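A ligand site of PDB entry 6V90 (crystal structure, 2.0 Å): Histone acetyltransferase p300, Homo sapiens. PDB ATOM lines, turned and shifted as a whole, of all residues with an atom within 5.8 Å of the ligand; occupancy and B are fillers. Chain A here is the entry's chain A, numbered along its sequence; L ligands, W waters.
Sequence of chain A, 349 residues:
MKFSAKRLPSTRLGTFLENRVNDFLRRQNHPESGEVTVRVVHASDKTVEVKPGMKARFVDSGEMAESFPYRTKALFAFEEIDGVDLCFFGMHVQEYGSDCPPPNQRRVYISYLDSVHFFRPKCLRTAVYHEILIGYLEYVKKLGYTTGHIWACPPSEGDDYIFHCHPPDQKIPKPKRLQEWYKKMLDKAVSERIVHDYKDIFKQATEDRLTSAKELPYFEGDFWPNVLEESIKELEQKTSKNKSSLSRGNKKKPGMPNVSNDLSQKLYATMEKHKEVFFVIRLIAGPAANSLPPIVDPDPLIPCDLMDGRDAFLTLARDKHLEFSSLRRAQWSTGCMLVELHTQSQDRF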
ATOM      1  N   PHE A  89     -29.646 -11.468 -25.819  1.00  0.00           N
ATOM      2  CA  PHE A  89     -30.930 -10.911 -25.364  1.00  0.00           C
ATOM      3  C   PHE A  89     -31.808 -12.009 -24.808  1.00  0.00           C
ATOM      4  O   PHE A  89     -31.832 -13.111 -25.324  1.00  0.00           O
ATOM      5  CB  PHE A  89     -31.670 -10.180 -26.526  1.00  0.00           C
ATOM      6  CG  PHE A  89     -32.945  -9.486 -26.080  1.00  0.00           C
ATOM      7  CD1 PHE A  89     -32.897  -8.232 -25.504  1.00  0.00           C
ATOM      8  CD2 PHE A  89     -34.180 -10.147 -26.174  1.00  0.00           C
ATOM      9  CE1 PHE A  89     -34.054  -7.617 -25.059  1.00  0.00           C
ATOM     10  CE2 PHE A  89     -35.345  -9.526 -25.737  1.00  0.00           C
ATOM     11  CZ  PHE A  89     -35.283  -8.260 -25.191  1.00  0.00           C
ATOM     12  N   LEU A 113     -36.234  -8.474 -18.650  1.00  0.00           N
ATOM     13  CA  LEU A 113     -35.453  -8.631 -19.851  1.00  0.00           C
ATOM     14  C   LEU A 113     -34.017  -8.332 -19.541  1.00  0.00           C
ATOM     15  O   LEU A 113     -33.698  -7.782 -18.481  1.00  0.00           O
ATOM     16  CB  LEU A 113     -35.977  -7.768 -20.964  1.00  0.00           C
ATOM     17  CG  LEU A 113     -36.193  -6.285 -20.783  1.00  0.00           C
ATOM     18  CD1 LEU A 113     -34.875  -5.568 -20.735  1.00  0.00           C
ATOM     19  CD2 LEU A 113     -37.033  -5.783 -21.947  1.00  0.00           C
ATOM     20  N   ASP A 114     -33.139  -8.758 -20.434  1.00  0.00           N
ATOM     21  CA  ASP A 114     -31.710  -8.610 -20.225  1.00  0.00           C
ATOM     22  C   ASP A 114     -30.954  -8.729 -21.521  1.00  0.00           C
ATOM     23  O   ASP A 114     -31.475  -9.198 -22.513  1.00  0.00           O
ATOM     24  CB  ASP A 114     -31.195  -9.670 -19.247  1.00  0.00           C
ATOM     25  CG  ASP A 114     -29.916  -9.219 -18.460  1.00  0.00           C
ATOM     26  OD1 ASP A 114     -29.287  -8.129 -18.757  1.00  0.00           O
ATOM     27  OD2 ASP A 114     -29.537  -9.983 -17.515  1.00  0.00           O
ATOM     28  N   SER A 115     -29.724  -8.242 -21.503  1.00  0.00           N
ATOM     29  CA  SER A 115     -28.877  -8.278 -22.678  1.00  0.00           C
ATOM     30  C   SER A 115     -27.415  -8.382 -22.280  1.00  0.00           C
ATOM     31  O   SER A 115     -27.055  -8.073 -21.125  1.00  0.00           O
ATOM     32  CB  SER A 115     -29.112  -7.049 -23.564  1.00  0.00           C
ATOM     33  OG  SER A 115     -28.496  -5.871 -23.056  1.00  0.00           O
ATOM     34  N   TYR A 129     -32.925  -4.775 -30.417  1.00  0.00           N
ATOM     35  CA  TYR A 129     -33.695  -4.934 -29.171  1.00  0.00           C
ATOM     36  C   TYR A 129     -35.118  -4.474 -29.400  1.00  0.00           C
ATOM     37  O   TYR A 129     -36.065  -5.156 -28.993  1.00  0.00           O
ATOM     38  CB  TYR A 129     -33.116  -4.161 -27.943  1.00  0.00           C
ATOM     39  CG  TYR A 129     -31.704  -4.523 -27.541  1.00  0.00           C
ATOM     40  CD1 TYR A 129     -31.246  -5.823 -27.660  1.00  0.00           C
ATOM     41  CD2 TYR A 129     -30.837  -3.553 -27.045  1.00  0.00           C
ATOM     42  CE1 TYR A 129     -29.957  -6.163 -27.310  1.00  0.00           C
ATOM     43  CE2 TYR A 129     -29.547  -3.869 -26.688  1.00  0.00           C
ATOM     44  CZ  TYR A 129     -29.104  -5.178 -26.822  1.00  0.00           C
ATOM     45  OH  TYR A 129     -27.841  -5.534 -26.491  1.00  0.00           O
ATOM     46  N   CYS A 153     -37.303  -0.649 -14.911  1.00  0.00           N
ATOM     47  CA  CYS A 153     -36.572  -0.786 -13.693  1.00  0.00           C
ATOM     48  C   CYS A 153     -35.224  -1.398 -13.977  1.00  0.00           C
ATOM     49  O   CYS A 153     -35.125  -2.594 -14.240  1.00  0.00           O
ATOM     50  CB  CYS A 153     -37.341  -1.627 -12.648  1.00  0.00           C
ATOM     51  SG  CYS A 153     -36.474  -1.696 -11.027  1.00  0.00           S
ATOM     52  N   PRO A 154     -34.157  -0.595 -13.873  1.00  0.00           N
ATOM     53  CA  PRO A 154     -32.884  -1.173 -14.132  1.00  0.00           C
ATOM     54  C   PRO A 154     -32.458  -2.074 -13.004  1.00  0.00           C
ATOM     55  O   PRO A 154     -32.838  -1.863 -11.849  1.00  0.00           O
ATOM     56  CB  PRO A 154     -31.927   0.012 -14.199  1.00  0.00           C
ATOM     57  CG  PRO A 154     -32.623   1.132 -13.648  1.00  0.00           C
ATOM     58  CD  PRO A 154     -34.080   0.810 -13.492  1.00  0.00           C
ATOM     59  N   PRO A 155     -31.626  -3.055 -13.330  1.00  0.00           N
ATOM     60  CA  PRO A 155     -30.982  -3.828 -12.251  1.00  0.00           C
ATOM     61  C   PRO A 155     -30.115  -2.911 -11.359  1.00  0.00           C
ATOM     62  O   PRO A 155     -29.621  -1.904 -11.836  1.00  0.00           O
ATOM     63  CB  PRO A 155     -30.091  -4.799 -13.012  1.00  0.00           C
ATOM     64  CG  PRO A 155     -29.839  -4.168 -14.340  1.00  0.00           C
ATOM     65  CD  PRO A 155     -31.013  -3.297 -14.653  1.00  0.00           C
ATOM     66  N   SER A 156     -29.918  -3.303 -10.100  1.00  0.00           N
ATOM     67  CA  SER A 156     -28.974  -2.610  -9.197  1.00  0.00           C
ATOM     68  C   SER A 156     -27.555  -2.859  -9.635  1.00  0.00           C
ATOM     69  O   SER A 156     -27.283  -3.857 -10.329  1.00  0.00           O
ATOM     70  CB  SER A 156     -29.112  -3.117  -7.776  1.00  0.00           C
ATOM     71  OG  SER A 156     -30.432  -2.959  -7.340  1.00  0.00           O
ATOM     72  N   GLU A 157     -26.648  -1.968  -9.184  1.00  0.00           N
ATOM     73  CA  GLU A 157     -25.206  -2.069  -9.495  1.00  0.00           C
ATOM     74  C   GLU A 157     -24.743  -3.463  -9.092  1.00  0.00           C
ATOM     75  O   GLU A 157     -25.146  -3.968  -8.055  1.00  0.00           O
ATOM     76  CB  GLU A 157     -24.389  -0.957  -8.795  1.00  0.00           C
ATOM     77  N   GLY A 158     -24.007  -4.109  -9.981  1.00  0.00           N
ATOM     78  CA  GLY A 158     -23.527  -5.467  -9.768  1.00  0.00           C
ATOM     79  C   GLY A 158     -24.511  -6.627  -9.794  1.00  0.00           C
ATOM     80  O   GLY A 158     -24.083  -7.759  -9.547  1.00  0.00           O
ATOM     81  N   ASP A 159     -25.800  -6.410 -10.076  1.00  0.00           N
ATOM     82  CA  ASP A 159     -26.781  -7.507 -10.115  1.00  0.00           C
ATOM     83  C   ASP A 159     -27.185  -7.870 -11.561  1.00  0.00           C
ATOM     84  O   ASP A 159     -26.975  -7.104 -12.490  1.00  0.00           O
ATOM     85  CB  ASP A 159     -28.001  -7.199  -9.244  1.00  0.00           C
ATOM     86  CG  ASP A 159     -28.661  -8.467  -8.713  1.00  0.00           C
ATOM     87  OD1 ASP A 159     -27.933  -9.369  -8.240  1.00  0.00           O
ATOM     88  OD2 ASP A 159     -29.905  -8.593  -8.773  1.00  0.00           O
ATOM     89  N   ASP A 160     -27.727  -9.061 -11.733  1.00  0.00           N
ATOM     90  CA  ASP A 160     -27.965  -9.649 -13.030  1.00  0.00           C
ATOM     91  C   ASP A 160     -29.376 -10.146 -13.003  1.00  0.00           C
ATOM     92  O   ASP A 160     -29.778 -10.890 -12.086  1.00  0.00           O
ATOM     93  CB  ASP A 160     -26.995 -10.795 -13.305  1.00  0.00           C
ATOM     94  CG  ASP A 160     -25.512 -10.343 -13.397  1.00  0.00           C
ATOM     95  OD1 ASP A 160     -25.185  -9.312 -14.029  1.00  0.00           O
ATOM     96  OD2 ASP A 160     -24.650 -11.081 -12.891  1.00  0.00           O
ATOM     97  N   TYR A 161     -30.152  -9.700 -13.974  1.00  0.00           N
ATOM     98  CA  TYR A 161     -31.507 -10.196 -14.136  1.00  0.00           C
ATOM     99  C   TYR A 161     -31.491 -11.611 -14.720  1.00  0.00           C
ATOM    100  O   TYR A 161     -32.101 -12.507 -14.150  1.00  0.00           O
ATOM    101  CB  TYR A 161     -32.348  -9.230 -15.004  1.00  0.00           C
ATOM    102  CG  TYR A 161     -32.910  -7.989 -14.301  1.00  0.00           C
ATOM    103  CD1 TYR A 161     -32.793  -7.779 -12.915  1.00  0.00           C
ATOM    104  CD2 TYR A 161     -33.551  -7.014 -15.034  1.00  0.00           C
ATOM    105  CE1 TYR A 161     -33.304  -6.663 -12.320  1.00  0.00           C
ATOM    106  CE2 TYR A 161     -34.099  -5.899 -14.434  1.00  0.00           C
ATOM    107  CZ  TYR A 161     -33.970  -5.714 -13.081  1.00  0.00           C
ATOM    108  OH  TYR A 161     -34.551  -4.593 -12.513  1.00  0.00           O
ATOM    109  N   HIS A 166     -22.027  -9.668 -16.244  1.00  0.00           N
ATOM    110  CA  HIS A 166     -22.036  -8.855 -17.443  1.00  0.00           C
ATOM    111  C   HIS A 166     -20.638  -8.255 -17.704  1.00  0.00           C
ATOM    112  O   HIS A 166     -19.801  -8.243 -16.813  1.00  0.00           O
ATOM    113  CB  HIS A 166     -23.068  -7.730 -17.258  1.00  0.00           C
ATOM    114  CG  HIS A 166     -24.463  -8.172 -17.524  1.00  0.00           C
ATOM    115  ND1 HIS A 166     -25.230  -8.816 -16.572  1.00  0.00           N
ATOM    116  CD2 HIS A 166     -25.237  -8.058 -18.631  1.00  0.00           C
ATOM    117  CE1 HIS A 166     -26.417  -9.085 -17.091  1.00  0.00           C
ATOM    118  NE2 HIS A 166     -26.451  -8.651 -18.338  1.00  0.00           N
ATOM    119  N   PRO A 167     -20.392  -7.731 -18.909  1.00  0.00           N
ATOM    120  CA  PRO A 167     -19.091  -7.090 -19.105  1.00  0.00           C
ATOM    121  C   PRO A 167     -18.886  -5.856 -18.194  1.00  0.00           C
ATOM    122  O   PRO A 167     -19.839  -5.062 -17.979  1.00  0.00           O
ATOM    123  CB  PRO A 167     -19.090  -6.687 -20.592  1.00  0.00           C
ATOM    124  CG  PRO A 167     -20.148  -7.554 -21.215  1.00  0.00           C
ATOM    125  CD  PRO A 167     -21.193  -7.742 -20.146  1.00  0.00           C
ATOM    126  N   PRO A 168     -17.671  -5.699 -17.665  1.00  0.00           N
ATOM    127  CA  PRO A 168     -17.463  -4.582 -16.744  1.00  0.00           C
ATOM    128  C   PRO A 168     -17.740  -3.209 -17.364  1.00  0.00           C
ATOM    129  O   PRO A 168     -18.120  -2.294 -16.631  1.00  0.00           O
ATOM    130  CB  PRO A 168     -15.989  -4.742 -16.297  1.00  0.00           C
ATOM    131  CG  PRO A 168     -15.373  -5.680 -17.279  1.00  0.00           C
ATOM    132  CD  PRO A 168     -16.482  -6.567 -17.755  1.00  0.00           C
ATOM    133  N   ASP A 169     -17.621  -3.076 -18.673  1.00  0.00           N
ATOM    134  CA  ASP A 169     -17.961  -1.809 -19.368  1.00  0.00           C
ATOM    135  C   ASP A 169     -19.375  -1.743 -19.966  1.00  0.00           C
ATOM    136  O   ASP A 169     -19.678  -0.773 -20.641  1.00  0.00           O
ATOM    137  CB  ASP A 169     -16.908  -1.496 -20.465  1.00  0.00           C
ATOM    138  CG  ASP A 169     -16.743  -2.623 -21.441  1.00  0.00           C
ATOM    139  OD1 ASP A 169     -17.130  -3.778 -21.091  1.00  0.00           O
ATOM    140  OD2 ASP A 169     -16.205  -2.373 -22.541  1.00  0.00           O
ATOM    141  N   GLN A 170     -20.222  -2.750 -19.748  1.00  0.00           N
ATOM    142  CA  GLN A 170     -21.651  -2.651 -20.114  1.00  0.00           C
ATOM    143  C   GLN A 170     -22.328  -1.904 -18.971  1.00  0.00           C
ATOM    144  O   GLN A 170     -22.510  -2.464 -17.862  1.00  0.00           O
ATOM    145  CB  GLN A 170     -22.332  -4.020 -20.348  1.00  0.00           C
ATOM    146  CG  GLN A 170     -23.801  -3.871 -20.752  1.00  0.00           C
ATOM    147  CD  GLN A 170     -24.488  -5.166 -21.074  1.00  0.00           C
ATOM    148  OE1 GLN A 170     -23.848  -6.160 -21.405  1.00  0.00           O
ATOM    149  NE2 GLN A 170     -25.817  -5.155 -20.981  1.00  0.00           N
ATOM    150  N   LYS A 171     -22.742  -0.666 -19.233  1.00  0.00           N
ATOM    151  CA  LYS A 171     -23.304   0.171 -18.178  1.00  0.00           C
ATOM    152  C   LYS A 171     -24.807  -0.051 -18.011  1.00  0.00           C
ATOM    153  O   LYS A 171     -25.558  -0.264 -18.966  1.00  0.00           O
ATOM    154  CB  LYS A 171     -22.913   1.637 -18.380  1.00  0.00           C
ATOM    155  CG  LYS A 171     -21.400   1.863 -18.188  1.00  0.00           C
ATOM    156  CD  LYS A 171     -20.954   3.301 -18.519  1.00  0.00           C
ATOM    157  CE  LYS A 171     -20.881   3.597 -20.027  1.00  0.00           C
ATOM    158  NZ  LYS A 171     -20.868   5.061 -20.368  1.00  0.00           N
ATOM    159  N   ILE A 172     -25.235  -0.007 -16.760  1.00  0.00           N
ATOM    160  CA  ILE A 172     -26.632  -0.089 -16.445  1.00  0.00           C
ATOM    161  C   ILE A 172     -27.223   1.275 -16.733  1.00  0.00           C
ATOM    162  O   ILE A 172     -26.790   2.216 -16.171  1.00  0.00           O
ATOM    163  CB  ILE A 172     -26.848  -0.451 -14.941  1.00  0.00           C
ATOM    164  CG1 ILE A 172     -26.274  -1.836 -14.686  1.00  0.00           C
ATOM    165  CG2 ILE A 172     -28.333  -0.436 -14.619  1.00  0.00           C
ATOM    166  CD1 ILE A 172     -26.052  -2.179 -13.226  1.00  0.00           C
ATOM    167  N   PRO A 173     -28.281   1.367 -17.541  1.00  0.00           N
ATOM    168  CA  PRO A 173     -28.877   2.698 -17.733  1.00  0.00           C
ATOM    169  C   PRO A 173     -29.567   3.263 -16.472  1.00  0.00           C
ATOM    170  O   PRO A 173     -30.193   2.530 -15.684  1.00  0.00           O
ATOM    171  CB  PRO A 173     -29.917   2.466 -18.805  1.00  0.00           C
ATOM    172  CG  PRO A 173     -30.218   1.044 -18.770  1.00  0.00           C
ATOM    173  CD  PRO A 173     -28.988   0.327 -18.289  1.00  0.00           C
ATOM    174  N   ARG A 177     -32.980   7.529 -18.743  1.00  0.00           N
ATOM    175  CA  ARG A 177     -32.487   6.958 -19.986  1.00  0.00           C
ATOM    176  C   ARG A 177     -33.292   5.713 -20.390  1.00  0.00           C
ATOM    177  O   ARG A 177     -33.668   5.548 -21.544  1.00  0.00           O
ATOM    178  CB  ARG A 177     -31.012   6.630 -19.837  1.00  0.00           C
ATOM    179  CG  ARG A 177     -30.405   6.037 -21.091  1.00  0.00           C
ATOM    180  CD  ARG A 177     -28.926   5.826 -20.889  1.00  0.00           C
ATOM    181  NE  ARG A 177     -28.393   4.829 -21.780  1.00  0.00           N
ATOM    182  CZ  ARG A 177     -28.233   4.999 -23.091  1.00  0.00           C
ATOM    183  NH1 ARG A 177     -28.532   6.167 -23.686  1.00  0.00           N
ATOM    184  NH2 ARG A 177     -27.714   4.005 -23.812  1.00  0.00           N
ATOM    185  N   LEU A 178     -33.534   4.829 -19.425  1.00  0.00           N
ATOM    186  CA  LEU A 178     -34.354   3.623 -19.665  1.00  0.00           C
ATOM    187  C   LEU A 178     -35.779   3.964 -20.068  1.00  0.00           C
ATOM    188  O   LEU A 178     -36.339   3.357 -20.961  1.00  0.00           O
ATOM    189  CB  LEU A 178     -34.376   2.737 -18.395  1.00  0.00           C
ATOM    190  CG  LEU A 178     -35.083   1.390 -18.480  1.00  0.00           C
ATOM    191  CD1 LEU A 178     -34.536   0.547 -19.594  1.00  0.00           C
ATOM    192  CD2 LEU A 178     -34.993   0.618 -17.158  1.00  0.00           C
ATOM    193  N   TRP A 181     -35.698   5.018 -23.509  1.00  0.00           N
ATOM    194  CA  TRP A 181     -35.540   3.904 -24.408  1.00  0.00           C
ATOM    195  C   TRP A 181     -36.874   3.170 -24.677  1.00  0.00           C
ATOM    196  O   TRP A 181     -37.202   2.774 -25.829  1.00  0.00           O
ATOM    197  CB  TRP A 181     -34.499   2.998 -23.779  1.00  0.00           C
ATOM    198  CG  TRP A 181     -34.014   1.833 -24.552  1.00  0.00           C
ATOM    199  CD1 TRP A 181     -32.846   1.778 -25.285  1.00  0.00           C
ATOM    200  CD2 TRP A 181     -34.550   0.503 -24.546  1.00  0.00           C
ATOM    201  NE1 TRP A 181     -32.677   0.501 -25.783  1.00  0.00           N
ATOM    202  CE2 TRP A 181     -33.698  -0.303 -25.322  1.00  0.00           C
ATOM    203  CE3 TRP A 181     -35.688  -0.087 -23.966  1.00  0.00           C
ATOM    204  CZ2 TRP A 181     -33.928  -1.662 -25.538  1.00  0.00           C
ATOM    205  CZ3 TRP A 181     -35.914  -1.444 -24.173  1.00  0.00           C
ATOM    206  CH2 TRP A 181     -35.046  -2.216 -24.951  1.00  0.00           C
ATOM    207  N   TYR A 182     -37.654   2.973 -23.640  1.00  0.00           N
ATOM    208  CA  TYR A 182     -38.966   2.341 -23.838  1.00  0.00           C
ATOM    209  C   TYR A 182     -39.912   3.263 -24.686  1.00  0.00           C
ATOM    210  O   TYR A 182     -40.614   2.756 -25.572  1.00  0.00           O
ATOM    211  CB  TYR A 182     -39.621   1.999 -22.485  1.00  0.00           C
ATOM    212  CG  TYR A 182     -39.076   0.768 -21.828  1.00  0.00           C
ATOM    213  CD1 TYR A 182     -39.254  -0.496 -22.414  1.00  0.00           C
ATOM    214  CD2 TYR A 182     -38.426   0.828 -20.592  1.00  0.00           C
ATOM    215  CE1 TYR A 182     -38.745  -1.640 -21.792  1.00  0.00           C
ATOM    216  CE2 TYR A 182     -37.966  -0.349 -19.954  1.00  0.00           C
ATOM    217  CZ  TYR A 182     -38.141  -1.574 -20.560  1.00  0.00           C
ATOM    218  OH  TYR A 182     -37.662  -2.737 -19.943  1.00  0.00           O
HETATM  219  C1  LIG L   1     -20.476  -4.938 -14.046  1.00  0.00           C
HETATM  220  N1  LIG L   1     -21.949  -5.071 -14.196  1.00  0.00           N
HETATM  221  C2  LIG L   1     -22.715  -4.837 -15.263  1.00  0.00           C
HETATM  222  N2  LIG L   1     -22.723  -5.486 -13.197  1.00  0.00           N
HETATM  223  C3  LIG L   1     -23.975  -5.497 -13.616  1.00  0.00           C
HETATM  224  C4  LIG L   1     -24.001  -5.066 -14.899  1.00  0.00           C
HETATM  225  C5  LIG L   1     -25.096  -5.031 -15.724  1.00  0.00           C
HETATM  226  C6  LIG L   1     -26.220  -5.847 -15.514  1.00  0.00           C
HETATM  227  N3  LIG L   1     -27.294  -5.844 -16.364  1.00  0.00           N
HETATM  228  C7  LIG L   1     -25.128  -4.259 -16.894  1.00  0.00           C
HETATM  229  C8  LIG L   1     -26.210  -4.258 -17.783  1.00  0.00           C
HETATM  230  C9  LIG L   1     -27.290  -5.098 -17.499  1.00  0.00           C
HETATM  231  N4  LIG L   1     -28.390  -5.217 -18.205  1.00  0.00           N
HETATM  232  C10 LIG L   1     -28.815  -4.420 -19.192  1.00  0.00           C
HETATM  233  O1  LIG L   1     -28.246  -3.471 -19.701  1.00  0.00           O
HETATM  234  C11 LIG L   1     -30.202  -4.791 -19.718  1.00  0.00           C
HETATM  235  C12 LIG L   1     -31.233  -4.141 -19.002  1.00  0.00           C
HETATM  236  C13 LIG L   1     -31.288  -2.751 -18.904  1.00  0.00           C
HETATM  237  C14 LIG L   1     -32.302  -2.073 -18.267  1.00  0.00           C
HETATM  238  C15 LIG L   1     -33.356  -2.822 -17.703  1.00  0.00           C
HETATM  239  C16 LIG L   1     -33.339  -4.212 -17.796  1.00  0.00           C
HETATM  240  C17 LIG L   1     -32.283  -4.861 -18.467  1.00  0.00           C
HETATM  241  N5  LIG L   1     -30.193  -4.479 -21.180  1.00  0.00           N
HETATM  242  C18 LIG L   1     -31.483  -4.706 -21.883  1.00  0.00           C
HETATM  243  C19 LIG L   1     -31.504  -3.950 -23.220  1.00  0.00           C
HETATM  244  C20 LIG L   1     -31.330  -2.576 -23.039  1.00  0.00           C
HETATM  245  C21 LIG L   1     -30.165  -1.889 -23.428  1.00  0.00           C
HETATM  246  C22 LIG L   1     -30.063  -0.503 -23.218  1.00  0.00           C
HETATM  247  C23 LIG L   1     -31.156   0.154 -22.654  1.00  0.00           C
HETATM  248  C24 LIG L   1     -31.175   1.521 -22.424  1.00  0.00           C
HETATM  249  N6  LIG L   1     -31.270   2.664 -22.195  1.00  0.00           N
HETATM  250  C25 LIG L   1     -32.299  -0.542 -22.284  1.00  0.00           C
HETATM  251  C26 LIG L   1     -32.379  -1.880 -22.467  1.00  0.00           C
HETATM  252  O   HOH W   1     -29.179  -7.749 -15.516  1.00  0.00           O
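Water W1 lies within hydrogen-bond range of the backbone NH of Tyr 161 (2.7 Å), a nitrogen (N3) of the ligand (2.8 Å) and the side-chain carboxylate of Asp 114 (3.0 Å).
O of Leu 113 touches C17 of the ligand, at 3.2 Å.
Tyr 129 touches the ligand.
Cys 153 touches the ligand (O to C15, 3.9 Å).
Pro 154 touches the ligand.
Pro 155 touches the ligand.
Gly 158 touches the ligand.
O of Asp 159 touches C6 of the ligand, at 3.4 Å.
Asp 160 touches the ligand.
CE2 of Tyr 161 touches C16 of the ligand, 3.8 Å away.
His 166 touches the ligand.
O of Pro 167 touches C2 of the ligand (3.96 Å).
Ile 172 touches the ligand.
Pro 173 touches the ligand.
Arg 177 touches the ligand (NE to N6, 3.6 Å).
CD1 of Leu 178 touches C25 of the ligand (3.7 Å).
Trp 181 touches the ligand.
Hydrophobic or aromatic side chains that line the ligand: Leu 113, Tyr 129, Pro 155, Tyr 161, His 166, Ile 172, Pro 173, Leu 178 and Trp 181.
Of the 26 residues printed, 19 come within 4 Å of the ligand.
The side-chain hydroxyl (OG) of Ser 115 sits at hydrogen-bond distance from a nitrogen (N5) of the ligand (2.9 Å).
N4 of the ligand sits at hydrogen-bond distance from OD1 of Asp 114, at 3.1 Å.
The side-chain amide nitrogen (NE2) of Gln 170 is in hydrogen-bond range of an oxygen (O1) of the ligand (3.2 Å).
The backbone carbonyl oxygen (O) of Ser 115 sits at hydrogen-bond distance from the side-chain amide nitrogen (NE2) of Gln 170, 3.2 Å away.
The backbone carbonyl oxygen (O) of Ser 115 lies within hydrogen-bond range of a ring nitrogen (NE2) of His 166, 2.9 Å away.
OD1 of Asp 114 is in hydrogen-bond range of NE2 of His 166, at 2.9 Å.
ND1 of His 166 lies within hydrogen-bond range of OD1 of Asp 160 (2.6 Å).
The backbone carbonyl oxygen of Cys 153 is in hydrogen-bond range of the side-chain hydroxyl of Tyr 161, 2.7 Å away.
The backbone carbonyl oxygen (O) of Pro 154 sits at hydrogen-bond distance from the side-chain hydroxyl (OH) of Tyr 161, 3.3 Å away.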
